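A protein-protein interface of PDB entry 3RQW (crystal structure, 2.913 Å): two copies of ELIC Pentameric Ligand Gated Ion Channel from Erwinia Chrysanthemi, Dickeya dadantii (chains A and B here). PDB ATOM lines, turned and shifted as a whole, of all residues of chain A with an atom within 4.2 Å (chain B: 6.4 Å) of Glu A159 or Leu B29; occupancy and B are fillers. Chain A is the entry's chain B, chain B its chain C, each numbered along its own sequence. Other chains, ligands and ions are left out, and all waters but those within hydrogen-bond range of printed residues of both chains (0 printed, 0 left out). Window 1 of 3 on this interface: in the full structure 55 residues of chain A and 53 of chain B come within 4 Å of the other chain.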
ATOM      1  N   ASP A 158     -21.751 -24.327  23.999  1.00  0.00           N
ATOM      2  CA  ASP A 158     -22.273 -24.291  25.364  1.00  0.00           C
ATOM      3  C   ASP A 158     -22.352 -25.672  26.009  1.00  0.00           C
ATOM      4  O   ASP A 158     -22.458 -26.693  25.334  1.00  0.00           O
ATOM      5  CB  ASP A 158     -23.658 -23.633  25.393  1.00  0.00           C
ATOM      6  CG  ASP A 158     -23.627 -22.161  25.000  1.00  0.00           C
ATOM      7  OD1 ASP A 158     -22.556 -21.517  25.091  1.00  0.00           O
ATOM      8  OD2 ASP A 158     -24.690 -21.640  24.608  1.00  0.00           O
ATOM      9  N   GLU A 159     -22.322 -25.692  27.331  1.00  0.00           N
ATOM     10  CA  GLU A 159     -22.347 -26.944  28.064  1.00  0.00           C
ATOM     11  C   GLU A 159     -23.749 -27.527  28.130  1.00  0.00           C
ATOM     12  O   GLU A 159     -23.931 -28.743  27.989  1.00  0.00           O
ATOM     13  CB  GLU A 159     -21.802 -26.717  29.467  1.00  0.00           C
ATOM     14  CG  GLU A 159     -21.612 -27.972  30.269  1.00  0.00           C
ATOM     15  CD  GLU A 159     -20.845 -27.696  31.551  1.00  0.00           C
ATOM     16  OE1 GLU A 159     -20.560 -28.661  32.304  1.00  0.00           O
ATOM     17  OE2 GLU A 159     -20.528 -26.504  31.792  1.00  0.00           O
ATOM     18  N   TRP A 160     -24.733 -26.648  28.336  1.00  0.00           N
ATOM     19  CA  TRP A 160     -26.138 -27.044  28.432  1.00  0.00           C
ATOM     20  C   TRP A 160     -26.985 -26.594  27.241  1.00  0.00           C
ATOM     21  O   TRP A 160     -26.822 -25.481  26.737  1.00  0.00           O
ATOM     22  CB  TRP A 160     -26.738 -26.506  29.727  1.00  0.00           C
ATOM     23  CG  TRP A 160     -26.133 -27.119  30.937  1.00  0.00           C
ATOM     24  CD1 TRP A 160     -25.080 -26.647  31.640  1.00  0.00           C
ATOM     25  CD2 TRP A 160     -26.539 -28.340  31.582  1.00  0.00           C
ATOM     26  NE1 TRP A 160     -24.797 -27.491  32.691  1.00  0.00           N
ATOM     27  CE2 TRP A 160     -25.679 -28.539  32.673  1.00  0.00           C
ATOM     28  CE3 TRP A 160     -27.543 -29.280  31.336  1.00  0.00           C
ATOM     29  CZ2 TRP A 160     -25.793 -29.637  33.527  1.00  0.00           C
ATOM     30  CZ3 TRP A 160     -27.655 -30.365  32.182  1.00  0.00           C
ATOM     31  CH2 TRP A 160     -26.783 -30.537  33.264  1.00  0.00           C
ATOM     32  N   ARG A 199     -27.850 -32.080  28.891  1.00  0.00           N
ATOM     33  CA  ARG A 199     -26.408 -31.890  28.901  1.00  0.00           C
ATOM     34  C   ARG A 199     -25.796 -32.221  27.542  1.00  0.00           C
ATOM     35  O   ARG A 199     -26.229 -33.169  26.866  1.00  0.00           O
ATOM     36  CB  ARG A 199     -25.760 -32.731  30.000  1.00  0.00           C
ATOM     37  CG  ARG A 199     -24.291 -32.412  30.219  1.00  0.00           C
ATOM     38  CD  ARG A 199     -23.626 -33.437  31.126  1.00  0.00           C
ATOM     39  NE  ARG A 199     -24.192 -33.452  32.472  1.00  0.00           N
ATOM     40  CZ  ARG A 199     -23.803 -32.644  33.451  1.00  0.00           C
ATOM     41  NH1 ARG A 199     -22.849 -31.748  33.239  1.00  0.00           N
ATOM     42  NH2 ARG A 199     -24.369 -32.726  34.642  1.00  0.00           N
ATOM     43  N   ASN A 200     -24.799 -31.428  27.151  1.00  0.00           N
ATOM     44  CA  ASN A 200     -24.079 -31.650  25.906  1.00  0.00           C
ATOM     45  C   ASN A 200     -23.098 -32.796  26.056  1.00  0.00           C
ATOM     46  O   ASN A 200     -21.982 -32.583  26.512  1.00  0.00           O
ATOM     47  CB  ASN A 200     -23.331 -30.383  25.498  1.00  0.00           C
ATOM     48  CG  ASN A 200     -22.542 -30.567  24.225  1.00  0.00           C
ATOM     49  OD1 ASN A 200     -21.668 -29.769  23.898  1.00  0.00           O
ATOM     50  ND2 ASN A 200     -22.844 -31.635  23.497  1.00  0.00           N
ATOM     51  N   ASN B  27     -11.967 -17.556  32.192  1.00  0.00           N
ATOM     52  CA  ASN B  27     -12.546 -18.798  32.690  1.00  0.00           C
ATOM     53  C   ASN B  27     -13.271 -19.529  31.577  1.00  0.00           C
ATOM     54  O   ASN B  27     -14.387 -19.180  31.234  1.00  0.00           O
ATOM     55  CB  ASN B  27     -13.506 -18.531  33.839  1.00  0.00           C
ATOM     56  CG  ASN B  27     -14.094 -19.806  34.419  1.00  0.00           C
ATOM     57  OD1 ASN B  27     -14.292 -20.805  33.715  1.00  0.00           O
ATOM     58  ND2 ASN B  27     -14.372 -19.779  35.719  1.00  0.00           N
ATOM     59  N   THR B  28     -12.635 -20.552  31.028  1.00  0.00           N
ATOM     60  CA  THR B  28     -13.163 -21.235  29.861  1.00  0.00           C
ATOM     61  C   THR B  28     -14.564 -21.801  30.071  1.00  0.00           C
ATOM     62  O   THR B  28     -15.452 -21.625  29.229  1.00  0.00           O
ATOM     63  CB  THR B  28     -12.231 -22.346  29.421  1.00  0.00           C
ATOM     64  OG1 THR B  28     -11.727 -23.014  30.581  1.00  0.00           O
ATOM     65  CG2 THR B  28     -11.083 -21.745  28.641  1.00  0.00           C
ATOM     66  N   LEU B  29     -14.766 -22.477  31.192  1.00  0.00           N
ATOM     67  CA  LEU B  29     -16.067 -23.070  31.487  1.00  0.00           C
ATOM     68  C   LEU B  29     -17.234 -22.062  31.569  1.00  0.00           C
ATOM     69  O   LEU B  29     -18.348 -22.342  31.098  1.00  0.00           O
ATOM     70  CB  LEU B  29     -15.974 -23.860  32.782  1.00  0.00           C
ATOM     71  CG  LEU B  29     -16.113 -25.343  32.518  1.00  0.00           C
ATOM     72  CD1 LEU B  29     -16.445 -26.043  33.821  1.00  0.00           C
ATOM     73  CD2 LEU B  29     -17.195 -25.533  31.472  1.00  0.00           C
ATOM     74  N   GLU B  30     -16.969 -20.901  32.176  1.00  0.00           N
ATOM     75  CA  GLU B  30     -17.967 -19.854  32.363  1.00  0.00           C
ATOM     76  C   GLU B  30     -17.974 -18.875  31.217  1.00  0.00           C
ATOM     77  O   GLU B  30     -18.841 -18.016  31.141  1.00  0.00           O
ATOM     78  CB  GLU B  30     -17.702 -19.071  33.642  1.00  0.00           C
ATOM     79  CG  GLU B  30     -17.775 -19.889  34.917  1.00  0.00           C
ATOM     80  CD  GLU B  30     -17.749 -19.036  36.182  1.00  0.00           C
ATOM     81  OE1 GLU B  30     -17.334 -17.831  36.119  1.00  0.00           O
ATOM     82  OE2 GLU B  30     -18.144 -19.605  37.238  1.00  0.00           O
ATOM     83  N   GLN B  31     -16.988 -18.985  30.339  1.00  0.00           N
ATOM     84  CA  GLN B  31     -16.831 -18.028  29.253  1.00  0.00           C
ATOM     85  C   GLN B  31     -16.837 -16.602  29.792  1.00  0.00           C
ATOM     86  O   GLN B  31     -17.607 -15.760  29.342  1.00  0.00           O
ATOM     87  CB  GLN B  31     -17.943 -18.214  28.226  1.00  0.00           C
ATOM     88  CG  GLN B  31     -18.067 -19.627  27.734  1.00  0.00           C
ATOM     89  CD  GLN B  31     -18.985 -19.748  26.553  1.00  0.00           C
ATOM     90  OE1 GLN B  31     -19.041 -18.861  25.702  1.00  0.00           O
ATOM     91  NE2 GLN B  31     -19.724 -20.850  26.493  1.00  0.00           N
ATOM     92  N   THR B  32     -15.972 -16.347  30.767  1.00  0.00           N
ATOM     93  CA  THR B  32     -15.813 -15.020  31.347  1.00  0.00           C
ATOM     94  C   THR B  32     -14.347 -14.615  31.347  1.00  0.00           C
ATOM     95  O   THR B  32     -13.476 -15.427  31.050  1.00  0.00           O
ATOM     96  CB  THR B  32     -16.340 -14.992  32.779  1.00  0.00           C
ATOM     97  OG1 THR B  32     -15.456 -15.725  33.642  1.00  0.00           O
ATOM     98  CG2 THR B  32     -17.709 -15.615  32.822  1.00  0.00           C
ATOM     99  N   PHE B 116     -13.586 -22.180  22.232  1.00  0.00           N
ATOM    100  CA  PHE B 116     -12.244 -22.676  22.514  1.00  0.00           C
ATOM    101  C   PHE B 116     -11.917 -23.934  21.713  1.00  0.00           C
ATOM    102  O   PHE B 116     -10.956 -24.641  22.020  1.00  0.00           O
ATOM    103  CB  PHE B 116     -12.068 -22.931  24.015  1.00  0.00           C
ATOM    104  CG  PHE B 116     -12.168 -21.688  24.848  1.00  0.00           C
ATOM    105  CD1 PHE B 116     -13.331 -21.395  25.544  1.00  0.00           C
ATOM    106  CD2 PHE B 116     -11.103 -20.797  24.918  1.00  0.00           C
ATOM    107  CE1 PHE B 116     -13.428 -20.241  26.303  1.00  0.00           C
ATOM    108  CE2 PHE B 116     -11.190 -19.646  25.674  1.00  0.00           C
ATOM    109  CZ  PHE B 116     -12.355 -19.363  26.366  1.00  0.00           C
ATOM    110  N   ARG B 255     -10.646 -26.616  31.361  1.00  0.00           N
ATOM    111  CA  ARG B 255     -11.848 -27.416  31.236  1.00  0.00           C
ATOM    112  C   ARG B 255     -12.782 -26.870  30.145  1.00  0.00           C
ATOM    113  O   ARG B 255     -12.977 -25.657  30.027  1.00  0.00           O
ATOM    114  CB  ARG B 255     -12.568 -27.495  32.582  1.00  0.00           C
ATOM    115  CG  ARG B 255     -12.242 -28.724  33.414  1.00  0.00           C
ATOM    116  CD  ARG B 255     -10.776 -28.756  33.791  1.00  0.00           C
ATOM    117  NE  ARG B 255     -10.491 -29.687  34.883  1.00  0.00           N
ATOM    118  CZ  ARG B 255      -9.331 -29.734  35.535  1.00  0.00           C
ATOM    119  NH1 ARG B 255      -8.344 -28.903  35.210  1.00  0.00           N
ATOM    120  NH2 ARG B 255      -9.157 -30.609  36.515  1.00  0.00           N
ATOM    121  N   LEU B 256     -13.340 -27.770  29.338  1.00  0.00           N
ATOM    122  CA  LEU B 256     -14.292 -27.390  28.296  1.00  0.00           C
ATOM    123  C   LEU B 256     -15.372 -28.446  28.157  1.00  0.00           C
ATOM    124  O   LEU B 256     -15.237 -29.555  28.656  1.00  0.00           O
ATOM    125  CB  LEU B 256     -13.589 -27.150  26.953  1.00  0.00           C
ATOM    126  CG  LEU B 256     -12.534 -26.034  26.931  1.00  0.00           C
ATOM    127  CD1 LEU B 256     -11.580 -26.169  25.757  1.00  0.00           C
ATOM    128  CD2 LEU B 256     -13.178 -24.669  26.917  1.00  0.00           C
ATOM    129  N   PRO B 257     -16.473 -28.091  27.503  1.00  0.00           N
ATOM    130  CA  PRO B 257     -17.586 -29.026  27.346  1.00  0.00           C
ATOM    131  C   PRO B 257     -17.487 -29.745  26.010  1.00  0.00           C
ATOM    132  O   PRO B 257     -18.404 -30.461  25.615  1.00  0.00           O
ATOM    133  CB  PRO B 257     -18.781 -28.095  27.315  1.00  0.00           C
ATOM    134  CG  PRO B 257     -18.242 -26.898  26.574  1.00  0.00           C
ATOM    135  CD  PRO B 257     -16.806 -26.751  26.992  1.00  0.00           C
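Among the printed residues, pairs that only touch across the chains: Glu A159 with Leu B29 (3.5 Å), Glu A159 with Pro B257 (3.8 Å) and Asn A200 with Pro B257 (3.8 Å).
Of the printed residues of chain B, Asp A158 touches Gln B31 (3.2 Å). Of the printed residues of chain B, Asn A200 touches Pro B257. Of chain A, only Glu A159 comes within 4 Å of Leu B29. Glu B30 touches none of the printed residues of chain A. Of the printed residues of chain A, Gln B31 touches Asp A158 (3.2 Å). Phe B116 touches none of the printed residues of chain A. Printed residues of chain A within 4 Å of Pro B257: Glu A159 and Asn A200. The nearest printed residue of chain A that does not touch Pro B257 is Asp A158 (4.3 Å).
O of Asp A158 sits close to OD1 of Asn A200, 3.5 Å away. The side-chain carboxylate (OE1) of Glu A159 lies within salt-bridge range of the guanidinium group (NH1) of Arg A199 (3.96 Å). The backbone carbonyl oxygen (O) of Glu A159 is in hydrogen-bond range of the backbone NH (N) of Asn A200. The side-chain amide oxygen of Asn B27 lies within hydrogen-bond range of the backbone NH of Leu B29 (3.1 Å).
No position is printed for both chains. Of the 4 pairs that touch across the chains among the printed residues, none has its exchanged pair printed and touching as well.
The side-chain carboxylate (OD1) of Asp A158 lies within hydrogen-bond range of the side-chain amide nitrogen (NE2) of Gln B31, 3.2 Å away.
Printed residues of chain B that touch a printed residue of chain A: Leu B29, Gln B31 and Pro B257. Hydrophobic or aromatic side chains of chain B that line the printed part of chain A: Leu B29 and Pro B257. Of the 5 printed residues of chain A, 3 touch a printed residue of chain B. Among the printed residues, 4 pairs touch across the chains. Among the printed residues, no Asp or Glu carboxylate lies within 4 Å of a Lys or Arg side-chain nitrogen of the other chain.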
